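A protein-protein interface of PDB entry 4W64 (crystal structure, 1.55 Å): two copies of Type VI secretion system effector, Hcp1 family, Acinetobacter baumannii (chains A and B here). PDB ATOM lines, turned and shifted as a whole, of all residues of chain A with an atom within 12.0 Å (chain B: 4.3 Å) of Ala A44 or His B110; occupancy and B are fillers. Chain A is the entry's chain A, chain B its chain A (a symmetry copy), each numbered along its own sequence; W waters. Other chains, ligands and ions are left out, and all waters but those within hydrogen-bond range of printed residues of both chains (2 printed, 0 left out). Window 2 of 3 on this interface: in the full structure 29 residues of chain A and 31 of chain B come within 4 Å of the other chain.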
ATOM      1  N   GLN A  40      -4.497  19.056 -19.674  1.00  0.00           N
ATOM      2  CA  GLN A  40      -3.511  18.315 -20.460  1.00  0.00           C
ATOM      3  C   GLN A  40      -2.513  17.636 -19.526  1.00  0.00           C
ATOM      4  O   GLN A  40      -1.744  18.310 -18.845  1.00  0.00           O
ATOM      5  CB  GLN A  40      -2.764  19.294 -21.383  1.00  0.00           C
ATOM      6  CG  GLN A  40      -1.600  18.684 -22.179  1.00  0.00           C
ATOM      7  CD  GLN A  40      -2.007  17.465 -22.996  1.00  0.00           C
ATOM      8  OE1 GLN A  40      -1.697  16.326 -22.632  1.00  0.00           O
ATOM      9  NE2 GLN A  40      -2.695  17.695 -24.111  1.00  0.00           N
ATOM     10  N   PRO A  41      -2.509  16.293 -19.484  1.00  0.00           N
ATOM     11  CA  PRO A  41      -1.625  15.560 -18.566  1.00  0.00           C
ATOM     12  C   PRO A  41      -0.178  15.380 -19.034  1.00  0.00           C
ATOM     13  O   PRO A  41       0.648  14.954 -18.214  1.00  0.00           O
ATOM     14  CB  PRO A  41      -2.301  14.187 -18.460  1.00  0.00           C
ATOM     15  CG  PRO A  41      -3.002  14.023 -19.774  1.00  0.00           C
ATOM     16  CD  PRO A  41      -3.487  15.411 -20.142  1.00  0.00           C
ATOM     17  N   LYS A  42       0.117  15.673 -20.299  1.00  0.00           N
ATOM     18  CA  LYS A  42       1.463  15.512 -20.853  1.00  0.00           C
ATOM     19  C   LYS A  42       2.558  16.084 -19.951  1.00  0.00           C
ATOM     20  O   LYS A  42       2.420  17.180 -19.408  1.00  0.00           O
ATOM     21  CB  LYS A  42       1.536  16.178 -22.228  1.00  0.00           C
ATOM     22  CG  LYS A  42       2.841  15.985 -22.977  1.00  0.00           C
ATOM     23  CD  LYS A  42       2.722  16.603 -24.355  1.00  0.00           C
ATOM     24  CE  LYS A  42       3.959  16.368 -25.190  1.00  0.00           C
ATOM     25  NZ  LYS A  42       3.787  16.978 -26.533  1.00  0.00           N
ATOM     26  N   SER A  43       3.639  15.328 -19.784  1.00  0.00           N
ATOM     27  CA  SER A  43       4.764  15.753 -18.947  1.00  0.00           C
ATOM     28  C   SER A  43       5.684  16.721 -19.683  1.00  0.00           C
ATOM     29  O   SER A  43       5.840  16.629 -20.903  1.00  0.00           O
ATOM     30  CB  SER A  43       5.569  14.524 -18.523  1.00  0.00           C
ATOM     31  OG  SER A  43       6.750  14.895 -17.837  1.00  0.00           O
ATOM     32  N   ALA A  44       6.287  17.652 -18.943  1.00  0.00           N
ATOM     33  CA  ALA A  44       7.307  18.543 -19.504  1.00  0.00           C
ATOM     34  C   ALA A  44       8.712  18.045 -19.194  1.00  0.00           C
ATOM     35  O   ALA A  44       9.691  18.636 -19.645  1.00  0.00           O
ATOM     36  CB  ALA A  44       7.125  19.973 -18.985  1.00  0.00           C
ATOM     37  N   THR A  45       8.823  16.960 -18.426  1.00  0.00           N
ATOM     38  CA  THR A  45      10.138  16.473 -18.016  1.00  0.00           C
ATOM     39  C   THR A  45      10.450  15.087 -18.562  1.00  0.00           C
ATOM     40  O   THR A  45      11.583  14.600 -18.430  1.00  0.00           O
ATOM     41  CB  THR A  45      10.293  16.462 -16.489  1.00  0.00           C
ATOM     42  OG1 THR A  45       9.199  15.738 -15.911  1.00  0.00           O
ATOM     43  CG2 THR A  45      10.294  17.885 -15.943  1.00  0.00           C
ATOM     44  N   SER A  46       9.446  14.453 -19.165  1.00  0.00           N
ATOM     45  CA  SER A  46       9.628  13.183 -19.855  1.00  0.00           C
ATOM     46  C   SER A  46       9.055  13.309 -21.255  1.00  0.00           C
ATOM     47  O   SER A  46       8.107  14.066 -21.475  1.00  0.00           O
ATOM     48  CB  SER A  46       8.910  12.054 -19.115  1.00  0.00           C
ATOM     49  OG  SER A  46       9.681  11.578 -18.032  1.00  0.00           O
ATOM     50  N   SER A  47       9.626  12.576 -22.201  1.00  0.00           N
ATOM     51  CA  SER A  47       9.100  12.574 -23.557  1.00  0.00           C
ATOM     52  C   SER A  47       9.113  11.169 -24.116  1.00  0.00           C
ATOM     53  O   SER A  47       9.948  10.346 -23.732  1.00  0.00           O
ATOM     54  CB  SER A  47       9.898  13.517 -24.457  1.00  0.00           C
ATOM     55  OG  SER A  47       9.621  14.866 -24.137  1.00  0.00           O
ATOM     56  N   SER A  48       8.175  10.883 -25.010  1.00  0.00           N
ATOM     57  CA  SER A  48       8.149   9.584 -25.656  1.00  0.00           C
ATOM     58  C   SER A  48       9.425   9.384 -26.457  1.00  0.00           C
ATOM     59  O   SER A  48       9.963  10.328 -27.026  1.00  0.00           O
ATOM     60  CB  SER A  48       6.945   9.471 -26.587  1.00  0.00           C
ATOM     61  OG  SER A  48       6.983   8.242 -27.292  1.00  0.00           O
ATOM     62  N   VAL A  49       9.910   8.148 -26.488  1.00  0.00           N
ATOM     63  CA  VAL A  49      11.044   7.791 -27.327  1.00  0.00           C
ATOM     64  C   VAL A  49      10.654   7.925 -28.798  1.00  0.00           C
ATOM     65  O   VAL A  49      11.480   8.278 -29.654  1.00  0.00           O
ATOM     66  CB  VAL A  49      11.521   6.358 -26.994  1.00  0.00           C
ATOM     67  CG1 VAL A  49      12.506   5.840 -28.030  1.00  0.00           C
ATOM     68  CG2 VAL A  49      12.145   6.329 -25.601  1.00  0.00           C
ATOM     69  N   GLY A  50       9.378   7.670 -29.084  1.00  0.00           N
ATOM     70  CA  GLY A  50       8.871   7.731 -30.442  1.00  0.00           C
ATOM     71  C   GLY A  50       7.853   8.841 -30.627  1.00  0.00           C
ATOM     72  O   GLY A  50       7.911   9.859 -29.938  1.00  0.00           O
ATOM     73  N   THR A  53       2.356   9.449 -27.723  1.00  0.00           N
ATOM     74  CA  THR A  53       2.139   9.807 -26.334  1.00  0.00           C
ATOM     75  C   THR A  53       0.806   9.176 -25.947  1.00  0.00           C
ATOM     76  O   THR A  53      -0.190   9.341 -26.653  1.00  0.00           O
ATOM     77  CB  THR A  53       2.064  11.336 -26.167  1.00  0.00           C
ATOM     78  OG1 THR A  53       3.093  11.958 -26.951  1.00  0.00           O
ATOM     79  CG2 THR A  53       2.231  11.734 -24.707  1.00  0.00           C
ATOM     80  N   GLU A  55      -1.414   9.337 -23.058  1.00  0.00           N
ATOM     81  CA  GLU A  55      -2.444  10.243 -22.574  1.00  0.00           C
ATOM     82  C   GLU A  55      -2.911  11.233 -23.629  1.00  0.00           C
ATOM     83  O   GLU A  55      -2.207  11.532 -24.595  1.00  0.00           O
ATOM     84  CB  GLU A  55      -1.919  11.026 -21.375  1.00  0.00           C
ATOM     85  CG  GLU A  55      -0.758  11.935 -21.734  1.00  0.00           C
ATOM     86  CD  GLU A  55       0.446  11.705 -20.857  1.00  0.00           C
ATOM     87  OE1 GLU A  55       0.254  11.488 -19.643  1.00  0.00           O
ATOM     88  OE2 GLU A  55       1.581  11.737 -21.380  1.00  0.00           O
ATOM     89  N   PHE B  85       6.618  24.673 -25.950  1.00  0.00           N
ATOM     90  CA  PHE B  85       7.252  25.937 -26.288  1.00  0.00           C
ATOM     91  C   PHE B  85       8.664  25.954 -25.771  1.00  0.00           C
ATOM     92  O   PHE B  85       8.940  25.473 -24.667  1.00  0.00           O
ATOM     93  CB  PHE B  85       6.453  27.084 -25.665  1.00  0.00           C
ATOM     94  CG  PHE B  85       5.031  27.134 -26.132  1.00  0.00           C
ATOM     95  CD1 PHE B  85       4.686  27.893 -27.247  1.00  0.00           C
ATOM     96  CD2 PHE B  85       4.039  26.386 -25.495  1.00  0.00           C
ATOM     97  CE1 PHE B  85       3.377  27.934 -27.698  1.00  0.00           C
ATOM     98  CE2 PHE B  85       2.724  26.412 -25.953  1.00  0.00           C
ATOM     99  CZ  PHE B  85       2.394  27.190 -27.058  1.00  0.00           C
ATOM    100  N   ASP B  86       9.581  26.488 -26.566  1.00  0.00           N
ATOM    101  CA  ASP B  86      10.971  26.517 -26.159  1.00  0.00           C
ATOM    102  C   ASP B  86      11.139  27.309 -24.868  1.00  0.00           C
ATOM    103  O   ASP B  86      11.892  26.909 -23.974  1.00  0.00           O
ATOM    104  CB  ASP B  86      11.827  27.136 -27.263  1.00  0.00           C
ATOM    105  CG  ASP B  86      11.776  26.342 -28.551  1.00  0.00           C
ATOM    106  OD1 ASP B  86      11.819  25.098 -28.475  1.00  0.00           O
ATOM    107  OD2 ASP B  86      11.682  26.961 -29.633  1.00  0.00           O
ATOM    108  N   LEU B 108      10.684  30.310 -18.227  1.00  0.00           N
ATOM    109  CA  LEU B 108      10.408  28.872 -18.159  1.00  0.00           C
ATOM    110  C   LEU B 108      10.888  28.222 -19.449  1.00  0.00           C
ATOM    111  O   LEU B 108      10.638  28.742 -20.541  1.00  0.00           O
ATOM    112  CB  LEU B 108       8.907  28.629 -18.007  1.00  0.00           C
ATOM    113  CG  LEU B 108       8.233  29.298 -16.820  1.00  0.00           C
ATOM    114  CD1 LEU B 108       6.731  29.002 -16.869  1.00  0.00           C
ATOM    115  CD2 LEU B 108       8.848  28.815 -15.508  1.00  0.00           C
ATOM    116  N   LYS B 109      11.592  27.098 -19.328  1.00  0.00           N
ATOM    117  CA  LYS B 109      12.142  26.398 -20.490  1.00  0.00           C
ATOM    118  C   LYS B 109      11.442  25.055 -20.710  1.00  0.00           C
ATOM    119  O   LYS B 109      11.247  24.285 -19.763  1.00  0.00           O
ATOM    120  CB  LYS B 109      13.650  26.191 -20.311  1.00  0.00           C
ATOM    121  CG  LYS B 109      14.350  25.582 -21.519  1.00  0.00           C
ATOM    122  CD  LYS B 109      15.875  25.555 -21.349  1.00  0.00           C
ATOM    123  CE  LYS B 109      16.459  26.957 -21.406  1.00  0.00           C
ATOM    124  NZ  LYS B 109      17.944  26.968 -21.307  1.00  0.00           N
ATOM    125  N   HIS B 110      11.069  24.794 -21.966  1.00  0.00           N
ATOM    126  CA  HIS B 110      10.384  23.557 -22.377  1.00  0.00           C
ATOM    127  C   HIS B 110       9.027  23.462 -21.687  1.00  0.00           C
ATOM    128  O   HIS B 110       8.854  22.752 -20.687  1.00  0.00           O
ATOM    129  CB  HIS B 110      11.266  22.321 -22.140  1.00  0.00           C
ATOM    130  CG  HIS B 110      10.726  21.064 -22.754  1.00  0.00           C
ATOM    131  ND1 HIS B 110      11.016  20.681 -24.046  1.00  0.00           N
ATOM    132  CD2 HIS B 110       9.916  20.105 -22.249  1.00  0.00           C
ATOM    133  CE1 HIS B 110      10.409  19.536 -24.310  1.00  0.00           C
ATOM    134  NE2 HIS B 110       9.730  19.167 -23.237  1.00  0.00           N
ATOM    135  N   VAL B 111       8.063  24.208 -22.229  1.00  0.00           N
ATOM    136  CA  VAL B 111       6.845  24.543 -21.508  1.00  0.00           C
ATOM    137  C   VAL B 111       5.618  24.037 -22.238  1.00  0.00           C
ATOM    138  O   VAL B 111       5.571  24.064 -23.469  1.00  0.00           O
ATOM    139  CB  VAL B 111       6.691  26.064 -21.382  1.00  0.00           C
ATOM    140  CG1 VAL B 111       5.613  26.398 -20.351  1.00  0.00           C
ATOM    141  CG2 VAL B 111       8.009  26.717 -21.034  1.00  0.00           C
ATOM    142  N   LEU B 112       4.636  23.578 -21.466  1.00  0.00           N
ATOM    143  CA  LEU B 112       3.345  23.147 -21.990  1.00  0.00           C
ATOM    144  C   LEU B 112       2.252  23.914 -21.264  1.00  0.00           C
ATOM    145  O   LEU B 112       2.403  24.248 -20.086  1.00  0.00           O
ATOM    146  CB  LEU B 112       3.124  21.662 -21.695  1.00  0.00           C
ATOM    147  CG  LEU B 112       3.973  20.558 -22.294  1.00  0.00           C
ATOM    148  CD1 LEU B 112       3.943  19.368 -21.365  1.00  0.00           C
ATOM    149  CD2 LEU B 112       3.393  20.172 -23.623  1.00  0.00           C
ATOM    150  N   LYS B 133       3.366  24.092 -17.249  1.00  0.00           N
ATOM    151  CA  LYS B 133       4.271  23.065 -16.734  1.00  0.00           C
ATOM    152  C   LYS B 133       5.555  23.178 -17.548  1.00  0.00           C
ATOM    153  O   LYS B 133       5.505  23.515 -18.738  1.00  0.00           O
ATOM    154  CB  LYS B 133       3.623  21.688 -16.912  1.00  0.00           C
ATOM    155  CG  LYS B 133       4.338  20.518 -16.267  1.00  0.00           C
ATOM    156  CD  LYS B 133       3.669  19.201 -16.684  1.00  0.00           C
ATOM    157  CE  LYS B 133       2.161  19.246 -16.516  1.00  0.00           C
ATOM    158  NZ  LYS B 133       1.511  17.944 -16.902  1.00  0.00           N
ATOM    159  N   TYR B 134       6.707  22.898 -16.937  1.00  0.00           N
ATOM    160  CA  TYR B 134       7.990  23.234 -17.567  1.00  0.00           C
ATOM    161  C   TYR B 134       9.110  22.323 -17.083  1.00  0.00           C
ATOM    162  O   TYR B 134       8.982  21.659 -16.050  1.00  0.00           O
ATOM    163  CB  TYR B 134       8.350  24.702 -17.248  1.00  0.00           C
ATOM    164  CG  TYR B 134       8.269  24.986 -15.761  1.00  0.00           C
ATOM    165  CD1 TYR B 134       9.369  24.790 -14.929  1.00  0.00           C
ATOM    166  CD2 TYR B 134       7.075  25.396 -15.182  1.00  0.00           C
ATOM    167  CE1 TYR B 134       9.290  25.020 -13.562  1.00  0.00           C
ATOM    168  CE2 TYR B 134       6.976  25.604 -13.810  1.00  0.00           C
ATOM    169  CZ  TYR B 134       8.086  25.417 -13.009  1.00  0.00           C
ATOM    170  OH  TYR B 134       7.996  25.632 -11.646  1.00  0.00           O
ATOM    171  N   ALA B 135      10.217  22.322 -17.818  1.00  0.00           N
ATOM    172  CA  ALA B 135      11.369  21.507 -17.455  1.00  0.00           C
ATOM    173  C   ALA B 135      12.378  22.270 -16.591  1.00  0.00           C
ATOM    174  O   ALA B 135      13.100  21.663 -15.795  1.00  0.00           O
ATOM    175  CB  ALA B 135      12.050  20.965 -18.701  1.00  0.00           C
ATOM    176  N   ALA B 169      17.077  22.486 -19.907  1.00  0.00           N
ATOM    177  CA  ALA B 169      16.132  21.379 -19.972  1.00  0.00           C
ATOM    178  C   ALA B 169      16.868  20.099 -20.326  1.00  0.00           C
ATOM    179  O   ALA B 169      16.610  19.045 -19.746  1.00  0.00           O
ATOM    180  CB  ALA B 169      15.044  21.661 -20.994  1.00  0.00           C
HETATM  181  O   HOH W   1       7.966  16.729 -22.794  1.00  0.00           O
HETATM  182  O   HOH W   2      -0.870  18.006 -15.856  1.00  0.00           O
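The backbone carbonyl oxygen (O) of Pro A41 sits at hydrogen-bond distance from the side-chain amino group (NZ) of Lys B133, 3.4 Å away.
The backbone carbonyl oxygen of Lys A42 lies within hydrogen-bond range of the side-chain amino group of Lys B133, 2.8 Å away.
N of Lys A42 is in hydrogen-bond range of OE1 of Gln A40 (3.0 Å).
OG of Ser A43 sits at hydrogen-bond distance from N of Thr A45, 3.0 Å away.
O of Asp B86 lies within hydrogen-bond range of N of His B110 (3.0 Å).
The backbone carbonyl oxygen (O) of Lys B109 sits at hydrogen-bond distance from the backbone NH (N) of Ala B135 (2.9 Å).
The backbone carbonyl oxygen (O) of His B110 is in hydrogen-bond range of the backbone NH (N) of Ala B135 (3.2 Å).
The backbone NH of Leu B112 lies within hydrogen-bond range of the backbone carbonyl oxygen of Lys B133 (2.9 Å).
Among the printed residues, merely in contact across the chains: Gln A40 with Lys B133 (3.8 Å), Lys A42 with Leu B112 (3.3 Å), Ser A43 with Leu B112 (3.4 Å), Ala A44 with His B110 (3.0 Å), Ala A44 with Leu B112 (3.8 Å), Ala A44 with Lys B133 (3.8 Å), Ala A44 with Tyr B134 (3.6 Å), Ala A44 with Ala B135 (3.4 Å) and Thr A45 with Tyr B134 (3.997 Å).
His B110 touches just one residue of chain A: Ala A44.
Leu B108 touches none of the printed residues of chain A.
No residue of chain A comes within 4 Å of Val B111.
Leu B112 touches just these residues of chain A: Lys A42, Ser A43 and Ala A44.
Of chain A, only Ala A44 (3.4 Å) comes within 4 Å of Ala B135.
No residue of chain A comes within 4 Å of Ala B169.
Of the printed residues of chain B, Gln A40 touches Lys B133 (3.8 Å).
Printed residues of chain B within 4 Å of Thr A45: Tyr B134.
Printed residues of chain B within 4 Å of Lys A42: Leu B112 and Lys B133.
Of the printed residues of chain B, Pro A41 touches Lys B133 (3.4 Å).
Of the printed residues of chain B, Ser A43 touches Leu B112.
Gly A50 touches none of the printed residues of chain B.
Ser A47 touches none of the printed residues of chain B.
The nearest printed residue of chain B that does not touch Ser A43 is Lys B133 (4.3 Å).
Printed residues of chain B that touch a printed residue of chain A: His B110, Leu B112, Lys B133, Tyr B134 and Ala B135.
Of the 13 printed residues of chain A, 6 touch a printed residue of chain B.
No position is printed for both chains.
Of the 11 pairs that touch across the chains among the printed residues, none has its exchanged pair printed and touching as well.
Water W2 bridges the side-chain amino group of Lys B133 (2.6 Å) and the backbone carbonyl oxygen of Gln A40 (3.1 Å).
Water W1 lies within hydrogen-bond range of OG of Ser A47 (2.8 Å), O of Ser A43 (2.8 Å), O of Ser A46 (3.0 Å) and NE2 of His B110 (3.0 Å).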
